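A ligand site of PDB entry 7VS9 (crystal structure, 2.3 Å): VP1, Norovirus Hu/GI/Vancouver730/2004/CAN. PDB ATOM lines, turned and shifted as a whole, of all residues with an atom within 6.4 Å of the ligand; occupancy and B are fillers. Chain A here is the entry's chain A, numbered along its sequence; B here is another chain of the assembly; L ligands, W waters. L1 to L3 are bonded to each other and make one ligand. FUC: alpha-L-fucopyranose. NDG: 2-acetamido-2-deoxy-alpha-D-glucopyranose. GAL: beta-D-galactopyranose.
Residues that only touch the ligand: Ala 122 of chain B (3.5 Å), Trp 167 (3.6 Å), Ala 172 (3.6 Å), Val 217 (3.7 Å) and Arg 171 (3.9 Å). Within 4 Å of the ligand: Asp 107, His 109, Trp 167, Ser 169, Asn 170, Arg 171, Ala 172, Val 217, Ala 122 of chain B and Asn 123 of chain B.
N of Asp 107 lies within hydrogen-bond range of O of Ser 169 (2.9 Å). N of His 109 sits at hydrogen-bond distance from O of Trp 167, 2.9 Å away. The backbone NH of Asn 170 lies within hydrogen-bond range of the backbone carbonyl oxygen of Val 217 (3.2 Å). The side-chain hydroxyl of Ser 169 is in hydrogen-bond range of a ring nitrogen (NE2) of His 109, at 2.6 Å. The side-chain carboxylate of Asp 107 is in hydrogen-bond range of the side-chain hydroxyl of Tyr 134, 2.6 Å away. The side-chain carboxylate of Asp 107 is in hydrogen-bond range of the side-chain amide nitrogen of Asn 130. OD1 of Asn 174 sits close to O of Ala 172. O of Asn 174 sits at hydrogen-bond distance from ND2 of Asn 170 (2.9 Å).
Water W3 lies within hydrogen-bond range of O of Glu 121 of chain B (2.7 Å), NH1 of Arg 175 (2.7 Å) and O4 of FUC L1 (2.8 Å). Water W5 bridges O3 of FUC L1 (2.9 Å) and N of Asn 173 (3.2 Å). Water W2 bridges the backbone NH (N) of Asp 124 of chain B (3.1 Å) and an oxygen (O1) of NDG L2 (3.2 Å).
An oxygen (O3) of GAL L3 is in hydrogen-bond range of the side-chain carboxylate (OD2) of Asp 107. NE2 of His 109 lies within hydrogen-bond range of O3 of GAL L3, at 2.9 Å. An oxygen (O3) of GAL L3 sits at hydrogen-bond distance from the side-chain hydroxyl (OG) of Ser 169 (2.9 Å). The backbone NH (N) of Asn 123 of chain B is in hydrogen-bond range of an oxygen (O5) of FUC L1. An oxygen (O4) of FUC L1 lies within hydrogen-bond range of the side-chain amide oxygen (OD1) of Asn 170 (2.9 Å). O4 of GAL L3 is in hydrogen-bond range of O of Asn 170 (2.7 Å).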
ATOM      1  N   ASP A 107      18.267 -14.183  -8.321  1.00  0.00           N
ATOM      2  CA  ASP A 107      17.613 -13.600  -7.149  1.00  0.00           C
ATOM      3  C   ASP A 107      18.576 -13.520  -5.983  1.00  0.00           C
ATOM      4  O   ASP A 107      19.372 -14.432  -5.746  1.00  0.00           O
ATOM      5  CB  ASP A 107      16.403 -14.442  -6.743  1.00  0.00           C
ATOM      6  CG  ASP A 107      15.233 -14.322  -7.717  1.00  0.00           C
ATOM      7  OD1 ASP A 107      15.270 -13.445  -8.617  1.00  0.00           O
ATOM      8  OD2 ASP A 107      14.275 -15.110  -7.586  1.00  0.00           O
ATOM      9  N   TRP A 108      18.488 -12.424  -5.241  1.00  0.00           N
ATOM     10  CA  TRP A 108      19.212 -12.267  -3.990  1.00  0.00           C
ATOM     11  C   TRP A 108      18.210 -12.527  -2.875  1.00  0.00           C
ATOM     12  O   TRP A 108      17.305 -11.719  -2.659  1.00  0.00           O
ATOM     13  CB  TRP A 108      19.823 -10.880  -3.801  1.00  0.00           C
ATOM     14  CG  TRP A 108      20.561 -10.287  -4.937  1.00  0.00           C
ATOM     15  CD1 TRP A 108      20.971 -10.882  -6.100  1.00  0.00           C
ATOM     16  CD2 TRP A 108      21.016  -8.927  -5.007  1.00  0.00           C
ATOM     17  NE1 TRP A 108      21.648  -9.970  -6.880  1.00  0.00           N
ATOM     18  CE2 TRP A 108      21.702  -8.772  -6.231  1.00  0.00           C
ATOM     19  CE3 TRP A 108      20.918  -7.821  -4.142  1.00  0.00           C
ATOM     20  CZ2 TRP A 108      22.262  -7.547  -6.622  1.00  0.00           C
ATOM     21  CZ3 TRP A 108      21.495  -6.613  -4.537  1.00  0.00           C
ATOM     22  CH2 TRP A 108      22.150  -6.490  -5.752  1.00  0.00           C
ATOM     23  N   HIS A 109      18.382 -13.638  -2.167  1.00  0.00           N
ATOM     24  CA  HIS A 109      17.600 -13.940  -0.980  1.00  0.00           C
ATOM     25  C   HIS A 109      18.316 -13.319   0.212  1.00  0.00           C
ATOM     26  O   HIS A 109      19.418 -13.752   0.593  1.00  0.00           O
ATOM     27  CB  HIS A 109      17.427 -15.456  -0.831  1.00  0.00           C
ATOM     28  CG  HIS A 109      16.811 -16.099  -2.035  1.00  0.00           C
ATOM     29  ND1 HIS A 109      15.465 -16.393  -2.118  1.00  0.00           N
ATOM     30  CD2 HIS A 109      17.361 -16.519  -3.200  1.00  0.00           C
ATOM     31  CE1 HIS A 109      15.218 -16.959  -3.286  1.00  0.00           C
ATOM     32  NE2 HIS A 109      16.349 -17.052  -3.954  1.00  0.00           N
ATOM     33  N   ASN A 130      13.445 -10.934  -0.864  1.00  0.00           N
ATOM     34  CA  ASN A 130      14.073 -11.329  -2.119  1.00  0.00           C
ATOM     35  C   ASN A 130      14.243 -10.082  -2.969  1.00  0.00           C
ATOM     36  O   ASN A 130      13.287  -9.328  -3.168  1.00  0.00           O
ATOM     37  CB  ASN A 130      13.202 -12.380  -2.826  1.00  0.00           C
ATOM     38  CG  ASN A 130      13.753 -12.796  -4.181  1.00  0.00           C
ATOM     39  OD1 ASN A 130      14.870 -12.423  -4.572  1.00  0.00           O
ATOM     40  ND2 ASN A 130      12.966 -13.577  -4.922  1.00  0.00           N
ATOM     41  N   TYR A 134      17.084  -7.931 -11.922  1.00  0.00           N
ATOM     42  CA  TYR A 134      16.518  -7.803 -13.263  1.00  0.00           C
ATOM     43  C   TYR A 134      15.123  -7.168 -13.254  1.00  0.00           C
ATOM     44  O   TYR A 134      14.550  -6.950 -14.320  1.00  0.00           O
ATOM     45  CB  TYR A 134      16.468  -9.188 -13.913  1.00  0.00           C
ATOM     46  CG  TYR A 134      15.775 -10.197 -13.038  1.00  0.00           C
ATOM     47  CD1 TYR A 134      14.383 -10.329 -13.071  1.00  0.00           C
ATOM     48  CD2 TYR A 134      16.492 -11.017 -12.149  1.00  0.00           C
ATOM     49  CE1 TYR A 134      13.724 -11.243 -12.280  1.00  0.00           C
ATOM     50  CE2 TYR A 134      15.828 -11.946 -11.342  1.00  0.00           C
ATOM     51  CZ  TYR A 134      14.440 -12.040 -11.419  1.00  0.00           C
ATOM     52  OH  TYR A 134      13.726 -12.933 -10.647  1.00  0.00           O
ATOM     53  N   TRP A 167      21.522 -16.305   0.267  1.00  0.00           N
ATOM     54  CA  TRP A 167      21.863 -17.155  -0.867  1.00  0.00           C
ATOM     55  C   TRP A 167      21.411 -16.486  -2.152  1.00  0.00           C
ATOM     56  O   TRP A 167      20.618 -15.539  -2.147  1.00  0.00           O
ATOM     57  CB  TRP A 167      21.258 -18.579  -0.727  1.00  0.00           C
ATOM     58  CG  TRP A 167      19.766 -18.668  -0.513  1.00  0.00           C
ATOM     59  CD1 TRP A 167      19.069 -18.206   0.581  1.00  0.00           C
ATOM     60  CD2 TRP A 167      18.795 -19.291  -1.374  1.00  0.00           C
ATOM     61  NE1 TRP A 167      17.721 -18.498   0.434  1.00  0.00           N
ATOM     62  CE2 TRP A 167      17.533 -19.164  -0.752  1.00  0.00           C
ATOM     63  CE3 TRP A 167      18.876 -19.944  -2.610  1.00  0.00           C
ATOM     64  CZ2 TRP A 167      16.353 -19.664  -1.322  1.00  0.00           C
ATOM     65  CZ3 TRP A 167      17.706 -20.447  -3.179  1.00  0.00           C
ATOM     66  CH2 TRP A 167      16.456 -20.303  -2.530  1.00  0.00           C
ATOM     67  N   LEU A 168      21.952 -16.992  -3.257  1.00  0.00           N
ATOM     68  CA  LEU A 168      21.588 -16.564  -4.598  1.00  0.00           C
ATOM     69  C   LEU A 168      20.948 -17.736  -5.332  1.00  0.00           C
ATOM     70  O   LEU A 168      21.234 -18.904  -5.034  1.00  0.00           O
ATOM     71  CB  LEU A 168      22.827 -16.088  -5.367  1.00  0.00           C
ATOM     72  CG  LEU A 168      23.618 -14.940  -4.737  1.00  0.00           C
ATOM     73  CD1 LEU A 168      25.040 -14.934  -5.272  1.00  0.00           C
ATOM     74  CD2 LEU A 168      22.944 -13.623  -5.030  1.00  0.00           C
ATOM     75  N   SER A 169      20.082 -17.444  -6.303  1.00  0.00           N
ATOM     76  CA  SER A 169      19.447 -18.522  -7.048  1.00  0.00           C
ATOM     77  C   SER A 169      19.215 -18.113  -8.495  1.00  0.00           C
ATOM     78  O   SER A 169      19.150 -16.916  -8.839  1.00  0.00           O
ATOM     79  CB  SER A 169      18.123 -18.977  -6.393  1.00  0.00           C
ATOM     80  OG  SER A 169      17.169 -17.926  -6.279  1.00  0.00           O
ATOM     81  N   ASN A 170      19.107 -19.133  -9.351  1.00  0.00           N
ATOM     82  CA  ASN A 170      18.877 -18.946 -10.777  1.00  0.00           C
ATOM     83  C   ASN A 170      17.482 -18.391 -11.048  1.00  0.00           C
ATOM     84  O   ASN A 170      16.541 -18.556 -10.258  1.00  0.00           O
ATOM     85  CB  ASN A 170      19.058 -20.272 -11.504  1.00  0.00           C
ATOM     86  CG  ASN A 170      18.132 -21.364 -10.966  1.00  0.00           C
ATOM     87  OD1 ASN A 170      18.326 -21.858  -9.850  1.00  0.00           O
ATOM     88  ND2 ASN A 170      17.105 -21.723 -11.737  1.00  0.00           N
ATOM     89  N   ARG A 171      17.350 -17.704 -12.184  1.00  0.00           N
ATOM     90  CA  ARG A 171      16.011 -17.384 -12.660  1.00  0.00           C
ATOM     91  C   ARG A 171      15.352 -18.660 -13.192  1.00  0.00           C
ATOM     92  O   ARG A 171      16.011 -19.671 -13.453  1.00  0.00           O
ATOM     93  CB  ARG A 171      16.080 -16.305 -13.752  1.00  0.00           C
ATOM     94  CG  ARG A 171      16.304 -14.894 -13.201  1.00  0.00           C
ATOM     95  CD  ARG A 171      16.683 -13.914 -14.316  1.00  0.00           C
ATOM     96  NE  ARG A 171      17.915 -14.310 -15.019  1.00  0.00           N
ATOM     97  CZ  ARG A 171      17.955 -14.838 -16.245  1.00  0.00           C
ATOM     98  NH1 ARG A 171      16.827 -15.029 -16.926  1.00  0.00           N
ATOM     99  NH2 ARG A 171      19.133 -15.177 -16.788  1.00  0.00           N
ATOM    100  N   ALA A 172      14.021 -18.603 -13.328  1.00  0.00           N
ATOM    101  CA  ALA A 172      13.279 -19.747 -13.832  1.00  0.00           C
ATOM    102  C   ALA A 172      13.777 -20.175 -15.206  1.00  0.00           C
ATOM    103  O   ALA A 172      14.000 -19.339 -16.098  1.00  0.00           O
ATOM    104  CB  ALA A 172      11.786 -19.399 -13.889  1.00  0.00           C
ATOM    105  N   ASN A 173      13.983 -21.492 -15.377  1.00  0.00           N
ATOM    106  CA  ASN A 173      14.461 -22.104 -16.627  1.00  0.00           C
ATOM    107  C   ASN A 173      15.817 -21.560 -17.079  1.00  0.00           C
ATOM    108  O   ASN A 173      16.131 -21.581 -18.276  1.00  0.00           O
ATOM    109  CB  ASN A 173      13.454 -21.945 -17.769  1.00  0.00           C
ATOM    110  CG  ASN A 173      12.029 -22.248 -17.345  1.00  0.00           C
ATOM    111  OD1 ASN A 173      11.170 -21.368 -17.372  1.00  0.00           O
ATOM    112  ND2 ASN A 173      11.774 -23.500 -16.959  1.00  0.00           N
ATOM    113  N   ASN A 174      16.642 -21.070 -16.157  1.00  0.00           N
ATOM    114  CA  ASN A 174      18.011 -20.666 -16.488  1.00  0.00           C
ATOM    115  C   ASN A 174      18.939 -21.140 -15.381  1.00  0.00           C
ATOM    116  O   ASN A 174      18.491 -21.569 -14.313  1.00  0.00           O
ATOM    117  CB  ASN A 174      18.136 -19.143 -16.662  1.00  0.00           C
ATOM    118  CG  ASN A 174      17.412 -18.617 -17.896  1.00  0.00           C
ATOM    119  OD1 ASN A 174      16.182 -18.466 -17.881  1.00  0.00           O
ATOM    120  ND2 ASN A 174      18.159 -18.318 -18.956  1.00  0.00           N
ATOM    121  N   ARG A 175      20.238 -21.056 -15.651  1.00  0.00           N
ATOM    122  CA  ARG A 175      21.251 -21.198 -14.621  1.00  0.00           C
ATOM    123  C   ARG A 175      21.705 -19.816 -14.150  1.00  0.00           C
ATOM    124  O   ARG A 175      21.545 -18.819 -14.862  1.00  0.00           O
ATOM    125  CB  ARG A 175      22.452 -21.991 -15.130  1.00  0.00           C
ATOM    126  CG  ARG A 175      22.137 -23.362 -15.706  1.00  0.00           C
ATOM    127  CD  ARG A 175      21.919 -24.373 -14.609  1.00  0.00           C
ATOM    128  NE  ARG A 175      20.538 -24.320 -14.123  1.00  0.00           N
ATOM    129  CZ  ARG A 175      20.085 -25.018 -13.082  1.00  0.00           C
ATOM    130  NH1 ARG A 175      18.799 -24.892 -12.723  1.00  0.00           N
ATOM    131  NH2 ARG A 175      20.900 -25.824 -12.395  1.00  0.00           N
ATOM    132  N   VAL A 217      22.608 -21.142  -5.630  1.00  0.00           N
ATOM    133  CA  VAL A 217      21.862 -22.336  -6.023  1.00  0.00           C
ATOM    134  C   VAL A 217      21.603 -22.298  -7.528  1.00  0.00           C
ATOM    135  O   VAL A 217      21.208 -21.257  -8.082  1.00  0.00           O
ATOM    136  CB  VAL A 217      20.546 -22.417  -5.218  1.00  0.00           C
ATOM    137  CG1 VAL A 217      19.623 -23.520  -5.761  1.00  0.00           C
ATOM    138  CG2 VAL A 217      20.854 -22.641  -3.735  1.00  0.00           C
ATOM    139  N   GLY A 218      21.840 -23.424  -8.193  1.00  0.00           N
ATOM    140  CA  GLY A 218      21.545 -23.521  -9.611  1.00  0.00           C
ATOM    141  C   GLY A 218      22.493 -22.730 -10.481  1.00  0.00           C
ATOM    142  O   GLY A 218      22.073 -22.185 -11.514  1.00  0.00           O
ATOM    143  N   GLU B 121      22.208 -27.565  -6.342  1.00  0.00           N
ATOM    144  CA  GLU B 121      21.726 -27.481  -7.709  1.00  0.00           C
ATOM    145  C   GLU B 121      20.326 -26.905  -7.786  1.00  0.00           C
ATOM    146  O   GLU B 121      19.953 -26.344  -8.823  1.00  0.00           O
ATOM    147  CB  GLU B 121      21.771 -28.864  -8.367  1.00  0.00           C
ATOM    148  CG  GLU B 121      23.186 -29.369  -8.629  1.00  0.00           C
ATOM    149  CD  GLU B 121      23.945 -28.467  -9.604  1.00  0.00           C
ATOM    150  OE1 GLU B 121      25.164 -28.254  -9.412  1.00  0.00           O
ATOM    151  OE2 GLU B 121      23.296 -27.970 -10.553  1.00  0.00           O
ATOM    152  N   ALA B 122      19.559 -26.990  -6.692  1.00  0.00           N
ATOM    153  CA  ALA B 122      18.169 -26.566  -6.655  1.00  0.00           C
ATOM    154  C   ALA B 122      17.749 -26.441  -5.200  1.00  0.00           C
ATOM    155  O   ALA B 122      18.421 -26.950  -4.300  1.00  0.00           O
ATOM    156  CB  ALA B 122      17.259 -27.544  -7.408  1.00  0.00           C
ATOM    157  N   ASN B 123      16.651 -25.695  -4.979  1.00  0.00           N
ATOM    158  CA  ASN B 123      15.909 -25.613  -3.718  1.00  0.00           C
ATOM    159  C   ASN B 123      16.537 -24.739  -2.632  1.00  0.00           C
ATOM    160  O   ASN B 123      17.720 -24.404  -2.672  1.00  0.00           O
ATOM    161  CB  ASN B 123      15.676 -27.015  -3.134  1.00  0.00           C
ATOM    162  CG  ASN B 123      15.035 -27.944  -4.128  1.00  0.00           C
ATOM    163  OD1 ASN B 123      13.972 -27.638  -4.698  1.00  0.00           O
ATOM    164  ND2 ASN B 123      15.684 -29.070  -4.383  1.00  0.00           N
ATOM    165  N   ASP B 124      15.719 -24.387  -1.652  1.00  0.00           N
ATOM    166  CA  ASP B 124      16.084 -23.517  -0.550  1.00  0.00           C
ATOM    167  C   ASP B 124      17.131 -24.182   0.348  1.00  0.00           C
ATOM    168  O   ASP B 124      16.819 -25.170   1.025  1.00  0.00           O
ATOM    169  CB  ASP B 124      14.823 -23.191   0.248  1.00  0.00           C
ATOM    170  CG  ASP B 124      15.064 -22.254   1.409  1.00  0.00           C
ATOM    171  OD1 ASP B 124      16.208 -21.809   1.606  1.00  0.00           O
ATOM    172  OD2 ASP B 124      14.083 -21.960   2.130  1.00  0.00           O
ATOM    173  N   PRO B 125      18.354 -23.647   0.423  1.00  0.00           N
ATOM    174  CA  PRO B 125      19.412 -24.263   1.242  1.00  0.00           C
ATOM    175  C   PRO B 125      19.478 -23.794   2.690  1.00  0.00           C
ATOM    176  O   PRO B 125      20.441 -24.151   3.380  1.00  0.00           O
ATOM    177  CB  PRO B 125      20.682 -23.855   0.496  1.00  0.00           C
ATOM    178  CG  PRO B 125      20.359 -22.438  -0.012  1.00  0.00           C
ATOM    179  CD  PRO B 125      18.821 -22.415  -0.236  1.00  0.00           C
HETATM  180  C1  FUC L   1      13.505 -24.733  -7.154  1.00  0.00           C
HETATM  181  C2  FUC L   1      14.142 -24.906  -8.525  1.00  0.00           C
HETATM  182  C3  FUC L   1      14.570 -23.545  -9.090  1.00  0.00           C
HETATM  183  C4  FUC L   1      15.597 -22.912  -8.147  1.00  0.00           C
HETATM  184  C5  FUC L   1      15.012 -22.832  -6.713  1.00  0.00           C
HETATM  185  C6  FUC L   1      16.010 -22.382  -5.657  1.00  0.00           C
HETATM  186  O2  FUC L   1      13.273 -25.549  -9.419  1.00  0.00           O
HETATM  187  O3  FUC L   1      15.177 -23.715 -10.378  1.00  0.00           O
HETATM  188  O4  FUC L   1      16.797 -23.695  -8.154  1.00  0.00           O
HETATM  189  O5  FUC L   1      14.420 -24.115  -6.262  1.00  0.00           O
HETATM  190  C1  NDG L   2       9.341 -24.537  -5.131  1.00  0.00           C
HETATM  191  C2  NDG L   2      10.311 -24.747  -6.312  1.00  0.00           C
HETATM  192  C3  NDG L   2      11.538 -23.813  -6.180  1.00  0.00           C
HETATM  193  C4  NDG L   2      11.081 -22.360  -5.954  1.00  0.00           C
HETATM  194  C5  NDG L   2      10.142 -22.331  -4.733  1.00  0.00           C
HETATM  195  C6  NDG L   2       9.540 -20.960  -4.422  1.00  0.00           C
HETATM  196  C7  NDG L   2      10.614 -26.889  -7.525  1.00  0.00           C
HETATM  197  C8  NDG L   2      11.143 -28.322  -7.418  1.00  0.00           C
HETATM  198  O5  NDG L   2       9.025 -23.154  -5.026  1.00  0.00           O
HETATM  199  O3  NDG L   2      12.322 -23.936  -7.362  1.00  0.00           O
HETATM  200  O4  NDG L   2      12.244 -21.557  -5.748  1.00  0.00           O
HETATM  201  O6  NDG L   2       8.814 -20.521  -5.554  1.00  0.00           O
HETATM  202  O7  NDG L   2      10.118 -26.442  -8.559  1.00  0.00           O
HETATM  203  N2  NDG L   2      10.747 -26.136  -6.390  1.00  0.00           N
HETATM  204  O1  NDG L   2       9.977 -24.996  -3.973  1.00  0.00           O
HETATM  205  C1  GAL L   3      12.278 -20.380  -6.568  1.00  0.00           C
HETATM  206  C2  GAL L   3      13.248 -19.394  -5.870  1.00  0.00           C
HETATM  207  C3  GAL L   3      13.435 -18.112  -6.699  1.00  0.00           C
HETATM  208  C4  GAL L   3      13.918 -18.486  -8.091  1.00  0.00           C
HETATM  209  C5  GAL L   3      12.895 -19.441  -8.707  1.00  0.00           C
HETATM  210  C6  GAL L   3      13.283 -19.935 -10.083  1.00  0.00           C
HETATM  211  O2  GAL L   3      12.757 -19.021  -4.593  1.00  0.00           O
HETATM  212  O3  GAL L   3      14.385 -17.206  -6.101  1.00  0.00           O
HETATM  213  O4  GAL L   3      15.177 -19.139  -8.045  1.00  0.00           O
HETATM  214  O5  GAL L   3      12.711 -20.645  -7.903  1.00  0.00           O
HETATM  215  O6  GAL L   3      12.503 -21.040 -10.432  1.00  0.00           O
HETATM  216  O   HOH W   1      12.811 -20.599  -2.227  1.00  0.00           O
HETATM  217  O   HOH W   2      12.665 -24.583  -2.221  1.00  0.00           O
HETATM  218  O   HOH W   3      17.848 -25.360 -10.212  1.00  0.00           O
HETATM  219  O   HOH W   4      14.310 -28.217  -9.765  1.00  0.00           O
HETATM  220  O   HOH W   5      13.839 -23.539 -12.987  1.00  0.00           O
